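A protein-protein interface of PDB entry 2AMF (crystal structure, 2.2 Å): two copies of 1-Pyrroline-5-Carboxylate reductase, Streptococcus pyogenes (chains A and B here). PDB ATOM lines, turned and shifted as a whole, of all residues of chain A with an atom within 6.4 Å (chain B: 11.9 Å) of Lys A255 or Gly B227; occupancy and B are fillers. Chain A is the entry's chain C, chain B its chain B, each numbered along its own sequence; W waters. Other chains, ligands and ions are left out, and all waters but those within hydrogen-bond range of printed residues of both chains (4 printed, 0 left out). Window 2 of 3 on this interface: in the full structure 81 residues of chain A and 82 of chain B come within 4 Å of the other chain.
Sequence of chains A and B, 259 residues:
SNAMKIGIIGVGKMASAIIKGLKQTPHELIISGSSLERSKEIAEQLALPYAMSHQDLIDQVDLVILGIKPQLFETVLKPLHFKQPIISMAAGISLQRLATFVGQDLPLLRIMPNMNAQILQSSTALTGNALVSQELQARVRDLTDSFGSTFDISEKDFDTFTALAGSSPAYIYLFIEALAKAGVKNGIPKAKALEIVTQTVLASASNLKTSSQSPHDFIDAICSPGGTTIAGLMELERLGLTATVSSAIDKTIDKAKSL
No residue of chain B comes within 4 Å of Gly A92.
Printed residues of chain B within 4 Å of Asp A250: Asn B186 (3.1 Å).
Of the printed residues of chain B, Lys A251 touches Glu B235.
Of the printed residues of chain B, Thr A252 touches Thr B228 and Gly B232.
No residue of chain B comes within 4 Å of Asp A254.
Ala A256 touches just one residue of chain B: Thr B228.
No residue of chain B comes within 4 Å of Lys A257.
Ser A258 touches none of the printed residues of chain B.
No residue of chain B comes within 4 Å of Leu A259.
Ile B222 touches none of the printed residues of chain A.
Gly B227 touches just one residue of chain A: Lys A255.
Printed residues of chain A within 4 Å of Thr B228: Thr A252, Lys A255 and Ala A256.
Of the printed residues of chain A, Ala B231 touches Lys A255.
Of the printed residues of chain A, Gly B232 touches Thr A252.
Water W1 bridges OD1 of Asp A250 (2.5 Å) and ND2 of Asn B186 (3.0 Å).
Water W3 bridges the side-chain amide oxygen of Asn B186 and the side-chain amino group of Lys A257.
Water W2 bridges NE2 of Gln A71 (2.9 Å) and O of Pro B225 (3.4 Å).
Water W4 bridges the side-chain amino group (NZ) of Lys A251 and the side-chain carboxylate (OE1) of Glu B235.
Along chain B the printed residues that touch a printed residue of chain A span positions 186 to 235.
Of the 12 printed residues of chain A, 7 touch a printed residue of chain B.
Printed residues of chain A that touch a printed residue of chain B: Gln A71, Asp A250, Lys A251, Thr A252, Ile A253, Lys A255 and Ala A256.
Hydrophobic or aromatic side chains of chain A that line the printed part of chain B: Ile A253 and Ala A256.
No position is printed for both chains.
Of the 11 pairs that touch across the chains among the printed residues, none has its exchanged pair printed and touching as well.
The side-chain hydroxyl of Ser A258 sits at hydrogen-bond distance from the backbone carbonyl oxygen of Lys A255 (3.3 Å).
CG of Lys A251 touches CG of Glu B235, at 3.7 Å.
CG2 of Thr A252 touches O of Thr B228, at 3.5 Å.
Thr A252 touches Gly B232 (OG1 to CA, 3.3 Å).
Ile A253 touches Asn B186.
Gly B226 touches Lys A255.
Lys A255 touches Gly B227 (CG to O, 3.4 Å).
Thr B228 touches Lys A255 (CA to CG, 3.7 Å).
CB of Ala B231 touches CB of Lys A255 (3.9 Å).
Ala A256 touches Thr B228 (N to CG2, 3.6 Å).
The backbone carbonyl oxygen (O) of Gly B226 lies close to the side-chain amide oxygen (OE1) of Gln A71.
OD1 of Asp A250 lies within hydrogen-bond range of ND2 of Asn B186 (3.1 Å).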
ATOM      1  N   GLN A  71      20.734 -20.629 -34.315  1.00  0.00           N
ATOM      2  CA  GLN A  71      21.228 -21.353 -35.478  1.00  0.00           C
ATOM      3  C   GLN A  71      21.847 -20.448 -36.546  1.00  0.00           C
ATOM      4  O   GLN A  71      22.743 -20.882 -37.252  1.00  0.00           O
ATOM      5  CB  GLN A  71      20.119 -22.206 -36.097  1.00  0.00           C
ATOM      6  CG  GLN A  71      19.761 -23.446 -35.307  1.00  0.00           C
ATOM      7  CD  GLN A  71      18.687 -23.217 -34.237  1.00  0.00           C
ATOM      8  OE1 GLN A  71      18.440 -24.091 -33.430  1.00  0.00           O
ATOM      9  NE2 GLN A  71      18.058 -22.060 -34.236  1.00  0.00           N
ATOM     10  N   GLY A  92      21.870 -20.808 -25.441  1.00  0.00           N
ATOM     11  CA  GLY A  92      23.006 -21.684 -25.617  1.00  0.00           C
ATOM     12  C   GLY A  92      24.205 -21.199 -26.413  1.00  0.00           C
ATOM     13  O   GLY A  92      25.028 -22.015 -26.804  1.00  0.00           O
ATOM     14  N   ASP A 250      15.814 -31.196 -17.964  1.00  0.00           N
ATOM     15  CA  ASP A 250      17.086 -31.782 -18.398  1.00  0.00           C
ATOM     16  C   ASP A 250      17.234 -31.792 -19.936  1.00  0.00           C
ATOM     17  O   ASP A 250      18.253 -31.343 -20.476  1.00  0.00           O
ATOM     18  CB  ASP A 250      17.254 -33.217 -17.848  1.00  0.00           C
ATOM     19  CG  ASP A 250      17.780 -33.261 -16.398  1.00  0.00           C
ATOM     20  OD1 ASP A 250      18.050 -32.210 -15.778  1.00  0.00           O
ATOM     21  OD2 ASP A 250      17.927 -34.374 -15.862  1.00  0.00           O
ATOM     22  N   LYS A 251      16.225 -32.318 -20.630  1.00  0.00           N
ATOM     23  CA  LYS A 251      16.128 -32.205 -22.092  1.00  0.00           C
ATOM     24  C   LYS A 251      16.228 -30.777 -22.619  1.00  0.00           C
ATOM     25  O   LYS A 251      16.782 -30.554 -23.687  1.00  0.00           O
ATOM     26  CB  LYS A 251      14.808 -32.789 -22.601  1.00  0.00           C
ATOM     27  CG  LYS A 251      14.803 -34.268 -22.756  1.00  0.00           C
ATOM     28  CD  LYS A 251      15.428 -34.710 -24.052  1.00  0.00           C
ATOM     29  CE  LYS A 251      15.812 -36.161 -23.934  1.00  0.00           C
ATOM     30  NZ  LYS A 251      16.284 -36.753 -25.235  1.00  0.00           N
ATOM     31  N   THR A 252      15.657 -29.823 -21.887  1.00  0.00           N
ATOM     32  CA  THR A 252      15.642 -28.423 -22.323  1.00  0.00           C
ATOM     33  C   THR A 252      17.072 -27.887 -22.294  1.00  0.00           C
ATOM     34  O   THR A 252      17.505 -27.191 -23.214  1.00  0.00           O
ATOM     35  CB  THR A 252      14.727 -27.577 -21.410  1.00  0.00           C
ATOM     36  OG1 THR A 252      13.432 -28.190 -21.324  1.00  0.00           O
ATOM     37  CG2 THR A 252      14.576 -26.133 -21.932  1.00  0.00           C
ATOM     38  N   ILE A 253      17.800 -28.267 -21.244  1.00  0.00           N
ATOM     39  CA  ILE A 253      19.172 -27.855 -20.994  1.00  0.00           C
ATOM     40  C   ILE A 253      20.168 -28.567 -21.942  1.00  0.00           C
ATOM     41  O   ILE A 253      21.092 -27.922 -22.468  1.00  0.00           O
ATOM     42  CB  ILE A 253      19.527 -28.092 -19.481  1.00  0.00           C
ATOM     43  CG1 ILE A 253      18.608 -27.253 -18.573  1.00  0.00           C
ATOM     44  CG2 ILE A 253      21.015 -27.786 -19.179  1.00  0.00           C
ATOM     45  CD1 ILE A 253      18.959 -27.331 -17.054  1.00  0.00           C
ATOM     46  N   ASP A 254      19.972 -29.875 -22.148  1.00  0.00           N
ATOM     47  CA  ASP A 254      20.681 -30.649 -23.157  1.00  0.00           C
ATOM     48  C   ASP A 254      20.589 -29.985 -24.544  1.00  0.00           C
ATOM     49  O   ASP A 254      21.581 -29.909 -25.274  1.00  0.00           O
ATOM     50  CB  ASP A 254      20.125 -32.078 -23.281  1.00  0.00           C
ATOM     51  CG  ASP A 254      20.474 -32.986 -22.095  1.00  0.00           C
ATOM     52  OD1 ASP A 254      21.334 -32.659 -21.245  1.00  0.00           O
ATOM     53  OD2 ASP A 254      19.854 -34.069 -22.019  1.00  0.00           O
ATOM     54  N   LYS A 255      19.402 -29.514 -24.911  1.00  0.00           N
ATOM     55  CA  LYS A 255      19.260 -28.782 -26.172  1.00  0.00           C
ATOM     56  C   LYS A 255      20.048 -27.460 -26.154  1.00  0.00           C
ATOM     57  O   LYS A 255      20.716 -27.135 -27.127  1.00  0.00           O
ATOM     58  CB  LYS A 255      17.788 -28.541 -26.518  1.00  0.00           C
ATOM     59  CG  LYS A 255      17.569 -27.930 -27.897  1.00  0.00           C
ATOM     60  CD  LYS A 255      17.947 -28.897 -29.014  1.00  0.00           C
ATOM     61  CE  LYS A 255      18.062 -28.162 -30.339  1.00  0.00           C
ATOM     62  NZ  LYS A 255      18.271 -29.091 -31.494  1.00  0.00           N
ATOM     63  N   ALA A 256      19.973 -26.710 -25.048  1.00  0.00           N
ATOM     64  CA  ALA A 256      20.734 -25.458 -24.919  1.00  0.00           C
ATOM     65  C   ALA A 256      22.236 -25.711 -25.046  1.00  0.00           C
ATOM     66  O   ALA A 256      22.928 -24.974 -25.743  1.00  0.00           O
ATOM     67  CB  ALA A 256      20.398 -24.728 -23.599  1.00  0.00           C
ATOM     68  N   LYS A 257      22.725 -26.759 -24.377  1.00  0.00           N
ATOM     69  CA  LYS A 257      24.119 -27.191 -24.464  1.00  0.00           C
ATOM     70  C   LYS A 257      24.578 -27.497 -25.905  1.00  0.00           C
ATOM     71  O   LYS A 257      25.613 -26.985 -26.343  1.00  0.00           O
ATOM     72  CB  LYS A 257      24.392 -28.380 -23.534  1.00  0.00           C
ATOM     73  CG  LYS A 257      24.432 -28.009 -22.058  1.00  0.00           C
ATOM     74  CD  LYS A 257      24.611 -29.250 -21.195  1.00  0.00           C
ATOM     75  CE  LYS A 257      24.573 -28.912 -19.702  1.00  0.00           C
ATOM     76  NZ  LYS A 257      24.253 -30.109 -18.836  1.00  0.00           N
ATOM     77  N   SER A 258      23.805 -28.281 -26.648  1.00  0.00           N
ATOM     78  CA  SER A 258      24.204 -28.669 -28.006  1.00  0.00           C
ATOM     79  C   SER A 258      24.109 -27.546 -29.054  1.00  0.00           C
ATOM     80  O   SER A 258      24.791 -27.593 -30.081  1.00  0.00           O
ATOM     81  CB  SER A 258      23.400 -29.887 -28.474  1.00  0.00           C
ATOM     82  OG  SER A 258      22.145 -29.498 -28.993  1.00  0.00           O
ATOM     83  N   LEU A 259      23.254 -26.555 -28.811  1.00  0.00           N
ATOM     84  CA  LEU A 259      23.181 -25.377 -29.670  1.00  0.00           C
ATOM     85  C   LEU A 259      24.456 -24.546 -29.536  1.00  0.00           C
ATOM     86  O   LEU A 259      25.115 -24.513 -28.478  1.00  0.00           O
ATOM     87  CB  LEU A 259      21.982 -24.496 -29.312  1.00  0.00           C
ATOM     88  CG  LEU A 259      20.571 -24.926 -29.726  1.00  0.00           C
ATOM     89  CD1 LEU A 259      19.497 -23.989 -29.142  1.00  0.00           C
ATOM     90  CD2 LEU A 259      20.457 -25.022 -31.243  1.00  0.00           C
ATOM     91  OXT LEU A 259      24.823 -23.867 -30.503  1.00  0.00           O
ATOM     92  N   ASN B 186      20.536 -28.718 -11.482  1.00  0.00           N
ATOM     93  CA  ASN B 186      21.318 -28.074 -12.510  1.00  0.00           C
ATOM     94  C   ASN B 186      22.106 -26.830 -12.027  1.00  0.00           C
ATOM     95  O   ASN B 186      22.538 -26.002 -12.831  1.00  0.00           O
ATOM     96  CB  ASN B 186      20.411 -27.801 -13.719  1.00  0.00           C
ATOM     97  CG  ASN B 186      20.092 -29.086 -14.501  1.00  0.00           C
ATOM     98  OD1 ASN B 186      20.967 -29.633 -15.170  1.00  0.00           O
ATOM     99  ND2 ASN B 186      18.849 -29.582 -14.393  1.00  0.00           N
ATOM    100  N   ILE B 219       1.949 -21.645 -26.281  1.00  0.00           N
ATOM    101  CA  ILE B 219       2.968 -22.687 -26.521  1.00  0.00           C
ATOM    102  C   ILE B 219       3.604 -22.564 -27.919  1.00  0.00           C
ATOM    103  O   ILE B 219       4.836 -22.595 -28.065  1.00  0.00           O
ATOM    104  CB  ILE B 219       2.411 -24.124 -26.242  1.00  0.00           C
ATOM    105  CG1 ILE B 219       2.167 -24.310 -24.732  1.00  0.00           C
ATOM    106  CG2 ILE B 219       3.359 -25.178 -26.782  1.00  0.00           C
ATOM    107  CD1 ILE B 219       1.292 -25.512 -24.367  1.00  0.00           C
ATOM    108  N   ASP B 220       2.764 -22.394 -28.939  1.00  0.00           N
ATOM    109  CA  ASP B 220       3.248 -22.114 -30.303  1.00  0.00           C
ATOM    110  C   ASP B 220       4.216 -20.920 -30.392  1.00  0.00           C
ATOM    111  O   ASP B 220       5.277 -21.025 -31.031  1.00  0.00           O
ATOM    112  CB  ASP B 220       2.070 -21.871 -31.256  1.00  0.00           C
ATOM    113  CG  ASP B 220       1.350 -23.146 -31.629  1.00  0.00           C
ATOM    114  OD1 ASP B 220       1.947 -24.243 -31.475  1.00  0.00           O
ATOM    115  OD2 ASP B 220       0.190 -23.047 -32.091  1.00  0.00           O
ATOM    116  N   ALA B 221       3.846 -19.796 -29.767  1.00  0.00           N
ATOM    117  CA  ALA B 221       4.710 -18.607 -29.739  1.00  0.00           C
ATOM    118  C   ALA B 221       6.060 -18.879 -29.070  1.00  0.00           C
ATOM    119  O   ALA B 221       7.096 -18.459 -29.571  1.00  0.00           O
ATOM    120  CB  ALA B 221       3.998 -17.434 -29.056  1.00  0.00           C
ATOM    121  N   ILE B 222       6.050 -19.612 -27.960  1.00  0.00           N
ATOM    122  CA  ILE B 222       7.273 -19.877 -27.183  1.00  0.00           C
ATOM    123  C   ILE B 222       8.193 -20.965 -27.807  1.00  0.00           C
ATOM    124  O   ILE B 222       9.416 -20.926 -27.652  1.00  0.00           O
ATOM    125  CB  ILE B 222       6.918 -20.196 -25.687  1.00  0.00           C
ATOM    126  CG1 ILE B 222       6.080 -19.062 -25.083  1.00  0.00           C
ATOM    127  CG2 ILE B 222       8.163 -20.448 -24.847  1.00  0.00           C
ATOM    128  CD1 ILE B 222       5.168 -19.488 -23.991  1.00  0.00           C
ATOM    129  N   CYS B 223       7.623 -21.928 -28.522  1.00  0.00           N
ATOM    130  CA  CYS B 223       8.462 -22.976 -29.110  1.00  0.00           C
ATOM    131  C   CYS B 223       9.178 -22.545 -30.394  1.00  0.00           C
ATOM    132  O   CYS B 223       8.758 -22.894 -31.505  1.00  0.00           O
ATOM    133  CB  CYS B 223       7.686 -24.283 -29.330  1.00  0.00           C
ATOM    134  SG  CYS B 223       7.072 -25.060 -27.825  1.00  0.00           S
ATOM    135  N   SER B 224      10.279 -21.809 -30.233  1.00  0.00           N
ATOM    136  CA  SER B 224      11.166 -21.495 -31.358  1.00  0.00           C
ATOM    137  C   SER B 224      11.526 -22.778 -32.086  1.00  0.00           C
ATOM    138  O   SER B 224      11.889 -23.775 -31.449  1.00  0.00           O
ATOM    139  CB  SER B 224      12.448 -20.773 -30.916  1.00  0.00           C
ATOM    140  OG  SER B 224      12.165 -19.754 -29.972  1.00  0.00           O
ATOM    141  N   PRO B 225      11.430 -22.759 -33.430  1.00  0.00           N
ATOM    142  CA  PRO B 225      11.731 -23.952 -34.220  1.00  0.00           C
ATOM    143  C   PRO B 225      13.166 -24.396 -34.010  1.00  0.00           C
ATOM    144  O   PRO B 225      14.092 -23.581 -34.133  1.00  0.00           O
ATOM    145  CB  PRO B 225      11.513 -23.487 -35.671  1.00  0.00           C
ATOM    146  CG  PRO B 225      10.614 -22.297 -35.559  1.00  0.00           C
ATOM    147  CD  PRO B 225      11.026 -21.624 -34.275  1.00  0.00           C
ATOM    148  N   GLY B 226      13.341 -25.679 -33.681  1.00  0.00           N
ATOM    149  CA  GLY B 226      14.656 -26.231 -33.423  1.00  0.00           C
ATOM    150  C   GLY B 226      15.236 -25.745 -32.093  1.00  0.00           C
ATOM    151  O   GLY B 226      16.445 -25.869 -31.860  1.00  0.00           O
ATOM    152  N   GLY B 227      14.378 -25.210 -31.226  1.00  0.00           N
ATOM    153  CA  GLY B 227      14.820 -24.557 -29.990  1.00  0.00           C
ATOM    154  C   GLY B 227      14.789 -25.446 -28.762  1.00  0.00           C
ATOM    155  O   GLY B 227      14.527 -26.660 -28.859  1.00  0.00           O
ATOM    156  N   THR B 228      15.020 -24.837 -27.599  1.00  0.00           N
ATOM    157  CA  THR B 228      15.104 -25.582 -26.345  1.00  0.00           C
ATOM    158  C   THR B 228      13.728 -25.986 -25.793  1.00  0.00           C
ATOM    159  O   THR B 228      13.594 -27.029 -25.154  1.00  0.00           O
ATOM    160  CB  THR B 228      15.903 -24.782 -25.267  1.00  0.00           C
ATOM    161  OG1 THR B 228      15.186 -23.594 -24.910  1.00  0.00           O
ATOM    162  CG2 THR B 228      17.274 -24.375 -25.801  1.00  0.00           C
ATOM    163  N   THR B 229      12.714 -25.168 -26.062  1.00  0.00           N
ATOM    164  CA  THR B 229      11.382 -25.324 -25.467  1.00  0.00           C
ATOM    165  C   THR B 229      10.607 -26.479 -26.086  1.00  0.00           C
ATOM    166  O   THR B 229       9.955 -27.244 -25.361  1.00  0.00           O
ATOM    167  CB  THR B 229      10.553 -24.016 -25.593  1.00  0.00           C
ATOM    168  OG1 THR B 229      11.286 -22.949 -24.996  1.00  0.00           O
ATOM    169  CG2 THR B 229       9.246 -24.137 -24.914  1.00  0.00           C
ATOM    170  N   ILE B 230      10.656 -26.585 -27.415  1.00  0.00           N
ATOM    171  CA  ILE B 230      10.063 -27.729 -28.088  1.00  0.00           C
ATOM    172  C   ILE B 230      10.749 -29.058 -27.688  1.00  0.00           C
ATOM    173  O   ILE B 230      10.108 -30.115 -27.668  1.00  0.00           O
ATOM    174  CB  ILE B 230       9.979 -27.534 -29.640  1.00  0.00           C
ATOM    175  CG1 ILE B 230       9.131 -28.641 -30.287  1.00  0.00           C
ATOM    176  CG2 ILE B 230      11.368 -27.435 -30.301  1.00  0.00           C
ATOM    177  CD1 ILE B 230       7.656 -28.656 -29.852  1.00  0.00           C
ATOM    178  N   ALA B 231      12.043 -29.016 -27.371  1.00  0.00           N
ATOM    179  CA  ALA B 231      12.709 -30.221 -26.862  1.00  0.00           C
ATOM    180  C   ALA B 231      12.107 -30.627 -25.503  1.00  0.00           C
ATOM    181  O   ALA B 231      11.731 -31.792 -25.294  1.00  0.00           O
ATOM    182  CB  ALA B 231      14.216 -30.016 -26.768  1.00  0.00           C
ATOM    183  N   GLY B 232      12.001 -29.670 -24.590  1.00  0.00           N
ATOM    184  CA  GLY B 232      11.369 -29.936 -23.298  1.00  0.00           C
ATOM    185  C   GLY B 232       9.899 -30.311 -23.433  1.00  0.00           C
ATOM    186  O   GLY B 232       9.432 -31.196 -22.734  1.00  0.00           O
ATOM    187  N   LEU B 233       9.164 -29.641 -24.321  1.00  0.00           N
ATOM    188  CA  LEU B 233       7.751 -29.953 -24.529  1.00  0.00           C
ATOM    189  C   LEU B 233       7.523 -31.393 -25.033  1.00  0.00           C
ATOM    190  O   LEU B 233       6.621 -32.091 -24.538  1.00  0.00           O
ATOM    191  CB  LEU B 233       7.090 -28.934 -25.478  1.00  0.00           C
ATOM    192  CG  LEU B 233       5.557 -29.034 -25.542  1.00  0.00           C
ATOM    193  CD1 LEU B 233       4.886 -28.288 -24.364  1.00  0.00           C
ATOM    194  CD2 LEU B 233       5.072 -28.503 -26.886  1.00  0.00           C
ATOM    195  N   MET B 234       8.317 -31.831 -26.009  1.00  0.00           N
ATOM    196  CA  MET B 234       8.208 -33.197 -26.512  1.00  0.00           C
ATOM    197  C   MET B 234       8.625 -34.228 -25.441  1.00  0.00           C
ATOM    198  O   MET B 234       8.119 -35.341 -25.445  1.00  0.00           O
ATOM    199  CB  MET B 234       8.962 -33.412 -27.833  1.00  0.00           C
ATOM    200  CG  MET B 234       8.213 -32.898 -29.132  1.00  0.00           C
ATOM    201  SD  MET B 234       6.518 -33.532 -29.437  1.00  0.00           S
ATOM    202  CE  MET B 234       5.655 -32.102 -28.815  1.00  0.00           C
ATOM    203  N   GLU B 235       9.502 -33.855 -24.510  1.00  0.00           N
ATOM    204  CA  GLU B 235       9.790 -34.732 -23.373  1.00  0.00           C
ATOM    205  C   GLU B 235       8.598 -34.835 -22.397  1.00  0.00           C
ATOM    206  O   GLU B 235       8.361 -35.901 -21.843  1.00  0.00           O
ATOM    207  CB  GLU B 235      11.067 -34.301 -22.650  1.00  0.00           C
ATOM    208  CG  GLU B 235      11.515 -35.227 -21.487  1.00  0.00           C
ATOM    209  CD  GLU B 235      12.003 -36.638 -21.902  1.00  0.00           C
ATOM    210  OE1 GLU B 235      11.902 -37.047 -23.108  1.00  0.00           O
ATOM    211  OE2 GLU B 235      12.507 -37.346 -20.992  1.00  0.00           O
ATOM    212  N   LEU B 236       7.865 -33.737 -22.204  1.00  0.00           N
ATOM    213  CA  LEU B 236       6.623 -33.742 -21.415  1.00  0.00           C
ATOM    214  C   LEU B 236       5.564 -34.659 -22.041  1.00  0.00           C
ATOM    215  O   LEU B 236       4.846 -35.349 -21.327  1.00  0.00           O
ATOM    216  CB  LEU B 236       6.051 -32.316 -21.267  1.00  0.00           C
ATOM    217  CG  LEU B 236       6.799 -31.338 -20.356  1.00  0.00           C
ATOM    218  CD1 LEU B 236       6.146 -29.962 -20.338  1.00  0.00           C
ATOM    219  CD2 LEU B 236       6.954 -31.892 -18.934  1.00  0.00           C
HETATM  220  O   HOH W   1      16.481 -31.429 -14.047  1.00  0.00           O
HETATM  221  O   HOH W   2      16.257 -21.985 -31.988  1.00  0.00           O
HETATM  222  O   HOH W   3      23.290 -28.707 -15.968  1.00  0.00           O
HETATM  223  O   HOH W   4      14.548 -38.766 -23.886  1.00  0.00           O
